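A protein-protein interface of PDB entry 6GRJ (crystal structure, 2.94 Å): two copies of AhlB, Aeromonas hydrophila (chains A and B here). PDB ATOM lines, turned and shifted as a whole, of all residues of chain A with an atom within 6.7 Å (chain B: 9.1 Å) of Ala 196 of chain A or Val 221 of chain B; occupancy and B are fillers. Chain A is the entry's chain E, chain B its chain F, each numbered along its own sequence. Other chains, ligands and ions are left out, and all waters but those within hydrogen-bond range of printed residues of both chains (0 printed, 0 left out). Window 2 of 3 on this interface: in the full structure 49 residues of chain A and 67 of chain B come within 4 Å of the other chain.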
ATOM      1  N   GLY A 191      -9.371   5.874  -8.766  1.00  0.00           N
ATOM      2  CA  GLY A 191      -8.149   5.632  -8.036  1.00  0.00           C
ATOM      3  C   GLY A 191      -8.298   5.864  -6.533  1.00  0.00           C
ATOM      4  O   GLY A 191      -7.799   5.083  -5.746  1.00  0.00           O
ATOM      5  N   ALA A 192      -8.990   6.934  -6.138  1.00  0.00           N
ATOM      6  CA  ALA A 192      -9.191   7.231  -4.719  1.00  0.00           C
ATOM      7  C   ALA A 192      -9.935   6.077  -4.031  1.00  0.00           C
ATOM      8  O   ALA A 192      -9.718   5.850  -2.846  1.00  0.00           O
ATOM      9  CB  ALA A 192      -9.938   8.534  -4.542  1.00  0.00           C
ATOM     10  N   PHE A 193     -10.806   5.377  -4.771  1.00  0.00           N
ATOM     11  CA  PHE A 193     -11.532   4.249  -4.233  1.00  0.00           C
ATOM     12  C   PHE A 193     -10.587   3.036  -4.125  1.00  0.00           C
ATOM     13  O   PHE A 193     -10.560   2.353  -3.068  1.00  0.00           O
ATOM     14  CB  PHE A 193     -12.755   3.860  -5.071  1.00  0.00           C
ATOM     15  CG  PHE A 193     -13.969   4.761  -5.132  1.00  0.00           C
ATOM     16  CD1 PHE A 193     -14.653   5.163  -3.990  1.00  0.00           C
ATOM     17  CD2 PHE A 193     -14.517   5.088  -6.367  1.00  0.00           C
ATOM     18  CE1 PHE A 193     -15.785   5.956  -4.084  1.00  0.00           C
ATOM     19  CE2 PHE A 193     -15.668   5.858  -6.460  1.00  0.00           C
ATOM     20  CZ  PHE A 193     -16.289   6.307  -5.318  1.00  0.00           C
ATOM     21  N   VAL A 194      -9.821   2.761  -5.193  1.00  0.00           N
ATOM     22  CA  VAL A 194      -8.868   1.631  -5.204  1.00  0.00           C
ATOM     23  C   VAL A 194      -7.794   1.848  -4.119  1.00  0.00           C
ATOM     24  O   VAL A 194      -7.490   0.950  -3.339  1.00  0.00           O
ATOM     25  CB  VAL A 194      -8.229   1.431  -6.595  1.00  0.00           C
ATOM     26  CG1 VAL A 194      -7.058   0.463  -6.557  1.00  0.00           C
ATOM     27  CG2 VAL A 194      -9.256   0.971  -7.620  1.00  0.00           C
ATOM     28  N   THR A 195      -7.223   3.058  -4.086  1.00  0.00           N
ATOM     29  CA  THR A 195      -6.214   3.445  -3.108  1.00  0.00           C
ATOM     30  C   THR A 195      -6.735   3.247  -1.681  1.00  0.00           C
ATOM     31  O   THR A 195      -5.953   2.899  -0.820  1.00  0.00           O
ATOM     32  CB  THR A 195      -5.783   4.906  -3.326  1.00  0.00           C
ATOM     33  OG1 THR A 195      -4.900   4.906  -4.446  1.00  0.00           O
ATOM     34  CG2 THR A 195      -5.095   5.541  -2.139  1.00  0.00           C
ATOM     35  N   ALA A 196      -8.036   3.477  -1.435  1.00  0.00           N
ATOM     36  CA  ALA A 196      -8.602   3.366  -0.084  1.00  0.00           C
ATOM     37  C   ALA A 196      -8.834   1.898   0.316  1.00  0.00           C
ATOM     38  O   ALA A 196      -8.695   1.581   1.516  1.00  0.00           O
ATOM     39  CB  ALA A 196      -9.880   4.145   0.014  1.00  0.00           C
ATOM     40  N   ILE A 197      -9.200   1.025  -0.641  1.00  0.00           N
ATOM     41  CA  ILE A 197      -9.424  -0.383  -0.322  1.00  0.00           C
ATOM     42  C   ILE A 197      -8.065  -1.088  -0.176  1.00  0.00           C
ATOM     43  O   ILE A 197      -7.847  -1.834   0.802  1.00  0.00           O
ATOM     44  CB  ILE A 197     -10.358  -1.101  -1.318  1.00  0.00           C
ATOM     45  CG1 ILE A 197      -9.833  -1.165  -2.753  1.00  0.00           C
ATOM     46  CG2 ILE A 197     -11.758  -0.513  -1.233  1.00  0.00           C
ATOM     47  CD1 ILE A 197     -10.433  -2.312  -3.551  1.00  0.00           C
ATOM     48  N   GLY A 198      -7.147  -0.824  -1.116  1.00  0.00           N
ATOM     49  CA  GLY A 198      -5.809  -1.399  -1.073  1.00  0.00           C
ATOM     50  C   GLY A 198      -5.068  -1.034   0.213  1.00  0.00           C
ATOM     51  O   GLY A 198      -4.245  -1.836   0.689  1.00  0.00           O
ATOM     52  N   ALA A 199      -5.358   0.161   0.762  1.00  0.00           N
ATOM     53  CA  ALA A 199      -4.691   0.713   1.961  1.00  0.00           C
ATOM     54  C   ALA A 199      -5.122  -0.008   3.239  1.00  0.00           C
ATOM     55  O   ALA A 199      -4.319  -0.161   4.169  1.00  0.00           O
ATOM     56  CB  ALA A 199      -4.961   2.198   2.086  1.00  0.00           C
ATOM     57  N   VAL A 200      -6.398  -0.414   3.303  1.00  0.00           N
ATOM     58  CA  VAL A 200      -6.889  -1.116   4.490  1.00  0.00           C
ATOM     59  C   VAL A 200      -6.979  -2.625   4.188  1.00  0.00           C
ATOM     60  O   VAL A 200      -7.763  -3.318   4.789  1.00  0.00           O
ATOM     61  CB  VAL A 200      -8.202  -0.493   5.017  1.00  0.00           C
ATOM     62  CG1 VAL A 200      -8.040   0.995   5.340  1.00  0.00           C
ATOM     63  CG2 VAL A 200      -9.373  -0.716   4.073  1.00  0.00           C
ATOM     64  N   ALA A 201      -6.156  -3.109   3.247  1.00  0.00           N
ATOM     65  CA  ALA A 201      -5.945  -4.531   2.935  1.00  0.00           C
ATOM     66  C   ALA A 201      -4.469  -4.874   3.252  1.00  0.00           C
ATOM     67  O   ALA A 201      -4.097  -6.045   3.413  1.00  0.00           O
ATOM     68  CB  ALA A 201      -6.319  -4.812   1.489  1.00  0.00           C
ATOM     69  N   VAL A 213      -2.456  -0.721  -4.327  1.00  0.00           N
ATOM     70  CA  VAL A 213      -2.281   0.638  -3.784  1.00  0.00           C
ATOM     71  C   VAL A 213      -1.425   1.457  -4.754  1.00  0.00           C
ATOM     72  O   VAL A 213      -1.566   2.687  -4.789  1.00  0.00           O
ATOM     73  CB  VAL A 213      -1.672   0.682  -2.371  1.00  0.00           C
ATOM     74  CG1 VAL A 213      -1.443   2.111  -1.881  1.00  0.00           C
ATOM     75  CG2 VAL A 213      -2.544  -0.056  -1.395  1.00  0.00           C
ATOM     76  N   GLY B 184     -19.560   7.767  -3.250  1.00  0.00           N
ATOM     77  CA  GLY B 184     -18.850   7.899  -1.970  1.00  0.00           C
ATOM     78  C   GLY B 184     -19.825   7.920  -0.795  1.00  0.00           C
ATOM     79  O   GLY B 184     -19.706   7.153   0.143  1.00  0.00           O
ATOM     80  N   LEU B 187     -21.351   4.516  -0.043  1.00  0.00           N
ATOM     81  CA  LEU B 187     -20.379   3.644   0.620  1.00  0.00           C
ATOM     82  C   LEU B 187     -20.262   4.005   2.106  1.00  0.00           C
ATOM     83  O   LEU B 187     -20.200   3.123   2.946  1.00  0.00           O
ATOM     84  CB  LEU B 187     -19.014   3.753  -0.049  1.00  0.00           C
ATOM     85  CG  LEU B 187     -18.877   3.000  -1.363  1.00  0.00           C
ATOM     86  CD1 LEU B 187     -17.490   3.224  -1.941  1.00  0.00           C
ATOM     87  CD2 LEU B 187     -19.135   1.518  -1.157  1.00  0.00           C
ATOM     88  N   VAL B 188     -20.240   5.297   2.425  1.00  0.00           N
ATOM     89  CA  VAL B 188     -20.133   5.724   3.800  1.00  0.00           C
ATOM     90  C   VAL B 188     -21.366   5.266   4.584  1.00  0.00           C
ATOM     91  O   VAL B 188     -21.217   4.703   5.663  1.00  0.00           O
ATOM     92  CB  VAL B 188     -19.924   7.241   3.919  1.00  0.00           C
ATOM     93  CG1 VAL B 188     -20.035   7.717   5.363  1.00  0.00           C
ATOM     94  CG2 VAL B 188     -18.596   7.659   3.279  1.00  0.00           C
ATOM     95  N   ILE B 189     -22.576   5.506   4.060  1.00  0.00           N
ATOM     96  CA  ILE B 189     -23.792   5.104   4.757  1.00  0.00           C
ATOM     97  C   ILE B 189     -23.823   3.576   4.852  1.00  0.00           C
ATOM     98  O   ILE B 189     -24.157   3.041   5.891  1.00  0.00           O
ATOM     99  CB  ILE B 189     -25.049   5.659   4.055  1.00  0.00           C
ATOM    100  CG1 ILE B 189     -25.105   7.178   4.144  1.00  0.00           C
ATOM    101  CG2 ILE B 189     -26.328   5.013   4.590  1.00  0.00           C
ATOM    102  CD1 ILE B 189     -26.169   7.788   3.261  1.00  0.00           C
ATOM    103  N   GLY B 191     -21.269   1.404   4.690  1.00  0.00           N
ATOM    104  CA  GLY B 191     -20.196   0.999   5.584  1.00  0.00           C
ATOM    105  C   GLY B 191     -20.529   1.233   7.044  1.00  0.00           C
ATOM    106  O   GLY B 191     -20.269   0.380   7.886  1.00  0.00           O
ATOM    107  N   ALA B 192     -21.104   2.396   7.366  1.00  0.00           N
ATOM    108  CA  ALA B 192     -21.453   2.698   8.754  1.00  0.00           C
ATOM    109  C   ALA B 192     -22.461   1.662   9.289  1.00  0.00           C
ATOM    110  O   ALA B 192     -22.483   1.380  10.480  1.00  0.00           O
ATOM    111  CB  ALA B 192     -21.973   4.096   8.866  1.00  0.00           C
ATOM    112  N   THR B 195     -20.270  -1.734   9.538  1.00  0.00           N
ATOM    113  CA  THR B 195     -19.423  -1.520  10.710  1.00  0.00           C
ATOM    114  C   THR B 195     -20.223  -1.700  12.016  1.00  0.00           C
ATOM    115  O   THR B 195     -19.707  -2.205  12.999  1.00  0.00           O
ATOM    116  CB  THR B 195     -18.732  -0.157  10.644  1.00  0.00           C
ATOM    117  OG1 THR B 195     -17.701  -0.206   9.641  1.00  0.00           O
ATOM    118  CG2 THR B 195     -18.142   0.257  11.974  1.00  0.00           C
ATOM    119  N   VAL B 213     -16.127  -6.107  10.063  1.00  0.00           N
ATOM    120  CA  VAL B 213     -15.910  -4.755  10.635  1.00  0.00           C
ATOM    121  C   VAL B 213     -14.783  -4.053   9.857  1.00  0.00           C
ATOM    122  O   VAL B 213     -14.722  -2.835   9.810  1.00  0.00           O
ATOM    123  CB  VAL B 213     -15.619  -4.762  12.147  1.00  0.00           C
ATOM    124  CG1 VAL B 213     -15.378  -3.335  12.658  1.00  0.00           C
ATOM    125  CG2 VAL B 213     -16.744  -5.432  12.932  1.00  0.00           C
ATOM    126  N   ILE B 214     -13.860  -4.829   9.284  1.00  0.00           N
ATOM    127  CA  ILE B 214     -12.815  -4.274   8.417  1.00  0.00           C
ATOM    128  C   ILE B 214     -13.483  -3.830   7.109  1.00  0.00           C
ATOM    129  O   ILE B 214     -13.390  -2.658   6.740  1.00  0.00           O
ATOM    130  CB  ILE B 214     -11.600  -5.209   8.215  1.00  0.00           C
ATOM    131  CG1 ILE B 214     -11.925  -6.544   7.542  1.00  0.00           C
ATOM    132  CG2 ILE B 214     -10.849  -5.388   9.538  1.00  0.00           C
ATOM    133  CD1 ILE B 214     -10.710  -7.260   6.970  1.00  0.00           C
ATOM    134  N   GLY B 215     -14.204  -4.748   6.460  1.00  0.00           N
ATOM    135  CA  GLY B 215     -14.927  -4.469   5.198  1.00  0.00           C
ATOM    136  C   GLY B 215     -15.818  -3.235   5.307  1.00  0.00           C
ATOM    137  O   GLY B 215     -15.919  -2.445   4.370  1.00  0.00           O
ATOM    138  N   GLY B 216     -16.465  -3.084   6.464  1.00  0.00           N
ATOM    139  CA  GLY B 216     -17.340  -1.963   6.768  1.00  0.00           C
ATOM    140  C   GLY B 216     -16.577  -0.656   6.883  1.00  0.00           C
ATOM    141  O   GLY B 216     -16.997   0.381   6.385  1.00  0.00           O
ATOM    142  N   VAL B 217     -15.436  -0.702   7.559  1.00  0.00           N
ATOM    143  CA  VAL B 217     -14.618   0.484   7.728  1.00  0.00           C
ATOM    144  C   VAL B 217     -13.863   0.764   6.410  1.00  0.00           C
ATOM    145  O   VAL B 217     -13.561   1.912   6.086  1.00  0.00           O
ATOM    146  CB  VAL B 217     -13.686   0.353   8.944  1.00  0.00           C
ATOM    147  CG1 VAL B 217     -12.716   1.526   9.033  1.00  0.00           C
ATOM    148  CG2 VAL B 217     -14.489   0.222  10.233  1.00  0.00           C
ATOM    149  N   ALA B 218     -13.559  -0.292   5.650  1.00  0.00           N
ATOM    150  CA  ALA B 218     -12.922  -0.129   4.350  1.00  0.00           C
ATOM    151  C   ALA B 218     -13.847   0.694   3.456  1.00  0.00           C
ATOM    152  O   ALA B 218     -13.420   1.651   2.829  1.00  0.00           O
ATOM    153  CB  ALA B 218     -12.603  -1.468   3.737  1.00  0.00           C
ATOM    154  N   MET B 219     -15.118   0.297   3.425  1.00  0.00           N
ATOM    155  CA  MET B 219     -16.153   0.986   2.670  1.00  0.00           C
ATOM    156  C   MET B 219     -16.199   2.466   3.065  1.00  0.00           C
ATOM    157  O   MET B 219     -16.181   3.339   2.200  1.00  0.00           O
ATOM    158  CB  MET B 219     -17.514   0.346   2.933  1.00  0.00           C
ATOM    159  CG  MET B 219     -17.761  -0.945   2.175  1.00  0.00           C
ATOM    160  SD  MET B 219     -19.407  -1.764   2.875  1.00  0.00           S
ATOM    161  CE  MET B 219     -19.004  -3.313   1.695  1.00  0.00           C
ATOM    162  N   MET B 220     -16.235   2.744   4.370  1.00  0.00           N
ATOM    163  CA  MET B 220     -16.278   4.114   4.855  1.00  0.00           C
ATOM    164  C   MET B 220     -15.062   4.937   4.425  1.00  0.00           C
ATOM    165  O   MET B 220     -15.184   6.119   4.103  1.00  0.00           O
ATOM    166  CB  MET B 220     -16.378   4.172   6.370  1.00  0.00           C
ATOM    167  CG  MET B 220     -17.739   3.667   6.848  1.00  0.00           C
ATOM    168  SD  MET B 220     -17.973   3.878   8.802  1.00  0.00           S
ATOM    169  CE  MET B 220     -17.804   5.840   9.077  1.00  0.00           C
ATOM    170  N   VAL B 221     -13.878   4.321   4.425  1.00  0.00           N
ATOM    171  CA  VAL B 221     -12.676   5.045   4.048  1.00  0.00           C
ATOM    172  C   VAL B 221     -12.719   5.312   2.535  1.00  0.00           C
ATOM    173  O   VAL B 221     -12.454   6.427   2.089  1.00  0.00           O
ATOM    174  CB  VAL B 221     -11.393   4.308   4.476  1.00  0.00           C
ATOM    175  CG1 VAL B 221     -10.133   4.983   3.948  1.00  0.00           C
ATOM    176  CG2 VAL B 221     -11.319   4.167   5.982  1.00  0.00           C
ATOM    177  N   ALA B 222     -13.041   4.272   1.763  1.00  0.00           N
ATOM    178  CA  ALA B 222     -13.170   4.382   0.304  1.00  0.00           C
ATOM    179  C   ALA B 222     -14.158   5.504  -0.035  1.00  0.00           C
ATOM    180  O   ALA B 222     -13.848   6.401  -0.805  1.00  0.00           O
ATOM    181  CB  ALA B 222     -13.592   3.061  -0.295  1.00  0.00           C
ATOM    182  N   GLY B 223     -15.339   5.437   0.572  1.00  0.00           N
ATOM    183  CA  GLY B 223     -16.402   6.442   0.408  1.00  0.00           C
ATOM    184  C   GLY B 223     -15.898   7.848   0.667  1.00  0.00           C
ATOM    185  O   GLY B 223     -16.048   8.703  -0.155  1.00  0.00           O
ATOM    186  N   ALA B 224     -15.276   8.081   1.824  1.00  0.00           N
ATOM    187  CA  ALA B 224     -14.727   9.397   2.170  1.00  0.00           C
ATOM    188  C   ALA B 224     -13.671   9.834   1.123  1.00  0.00           C
ATOM    189  O   ALA B 224     -13.492  11.039   0.854  1.00  0.00           O
ATOM    190  CB  ALA B 224     -14.173   9.364   3.559  1.00  0.00           C
ATOM    191  N   GLY B 225     -12.972   8.837   0.565  1.00  0.00           N
ATOM    192  CA  GLY B 225     -12.010   9.065  -0.500  1.00  0.00           C
ATOM    193  C   GLY B 225     -12.705   9.601  -1.752  1.00  0.00           C
ATOM    194  O   GLY B 225     -12.396  10.674  -2.255  1.00  0.00           O
ATOM    195  N   GLY B 226     -13.692   8.845  -2.222  1.00  0.00           N
ATOM    196  CA  GLY B 226     -14.516   9.201  -3.387  1.00  0.00           C
ATOM    197  C   GLY B 226     -15.157  10.570  -3.241  1.00  0.00           C
ATOM    198  O   GLY B 226     -15.202  11.335  -4.179  1.00  0.00           O
ATOM    199  N   ILE B 227     -15.627  10.893  -2.039  1.00  0.00           N
ATOM    200  CA  ILE B 227     -16.266  12.154  -1.759  1.00  0.00           C
ATOM    201  C   ILE B 227     -15.259  13.284  -1.907  1.00  0.00           C
ATOM    202  O   ILE B 227     -15.542  14.238  -2.597  1.00  0.00           O
ATOM    203  CB  ILE B 227     -16.910  12.155  -0.362  1.00  0.00           C
ATOM    204  CG1 ILE B 227     -18.124  11.233  -0.367  1.00  0.00           C
ATOM    205  CG2 ILE B 227     -17.259  13.563   0.089  1.00  0.00           C
ATOM    206  CD1 ILE B 227     -18.783  11.011   0.946  1.00  0.00           C
ATOM    207  N   THR B 228     -14.107  13.184  -1.248  1.00  0.00           N
ATOM    208  CA  THR B 228     -13.147  14.292  -1.301  1.00  0.00           C
ATOM    209  C   THR B 228     -12.500  14.333  -2.703  1.00  0.00           C
ATOM    210  O   THR B 228     -12.194  15.419  -3.203  1.00  0.00           O
ATOM    211  CB  THR B 228     -12.191  14.271  -0.101  1.00  0.00           C
ATOM    212  OG1 THR B 228     -11.482  13.045  -0.162  1.00  0.00           O
ATOM    213  CG2 THR B 228     -12.882  14.383   1.245  1.00  0.00           C
ATOM    214  N   ALA B 229     -12.357  13.177  -3.362  1.00  0.00           N
ATOM    215  CA  ALA B 229     -11.806  13.128  -4.730  1.00  0.00           C
ATOM    216  C   ALA B 229     -12.784  13.807  -5.701  1.00  0.00           C
ATOM    217  O   ALA B 229     -12.415  14.660  -6.502  1.00  0.00           O
ATOM    218  CB  ALA B 229     -11.520  11.709  -5.147  1.00  0.00           C
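The side-chain hydroxyl of Thr 228 of chain B is in hydrogen-bond range of the backbone carbonyl oxygen of Gly 225 of chain B, at 3.3 Å.
Among the printed residues, pairs that only touch across the chains: Ala 196 of chain A with Ala 222 of chain B (3.3 Å), Val 200 of chain A with Ala 218 of chain B (3.3 Å), Phe 193 of chain A with Ala 222 of chain B (3.5 Å), Phe 193 of chain A with Gly 226 of chain B (3.6 Å), Ala 192 of chain A with Ala 229 of chain B (3.6 Å), Phe 193 of chain A with Leu 187 of chain B (3.9 Å), Ala 196 of chain A with Val 221 of chain B (3.97 Å) and Ala 192 of chain A with Gly 225 of chain B (3.98 Å).
Of chain B, only Val 221 and Ala 222 come within 4 Å of Ala 196 of chain A.
Val 221 of chain B touches just one residue of chain A: Ala 196.
Thr 195 of chain A touches none of the printed residues of chain B.
Of the printed residues of chain A, Ala 229 of chain B touches Ala 192.
Of the printed residues of chain B, Ala 192 of chain A touches Gly 225 (3.98 Å) and Ala 229 (3.6 Å).
Met 219 of chain B touches none of the printed residues of chain A.
Ala 199 of chain A touches none of the printed residues of chain B.
The nearest residue of chain A that does not touch Val 221 of chain B is Val 200 of chain A (4.6 Å).
Of the 24 printed residues of chain B, 7 touch a printed residue of chain A.
Hydrophobic or aromatic side chains of chain B that line the printed part of chain A: Leu 187, Ala 218, Ala 222 and Ala 229.
Along chain B the printed residues that touch a printed residue of chain A span positions 187 to 229.
Of the 12 printed residues of chain A, 4 touch a printed residue of chain B.
Printed residues of chain A that touch a printed residue of chain B: Ala 192, Phe 193, Ala 196 and Val 200.
Hydrophobic or aromatic side chains of chain A that line the printed part of chain B: Ala 192, Phe 193, Ala 196 and Val 200.
Among the printed residues, 8 pairs touch across the chains.
Among the printed residues, no Asp or Glu carboxylate lies within 4 Å of a Lys or Arg side-chain nitrogen of the other chain.
4 positions are printed for both chains.
Of the 8 pairs that touch across the chains among the printed residues, none has its exchanged pair printed and touching as well.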
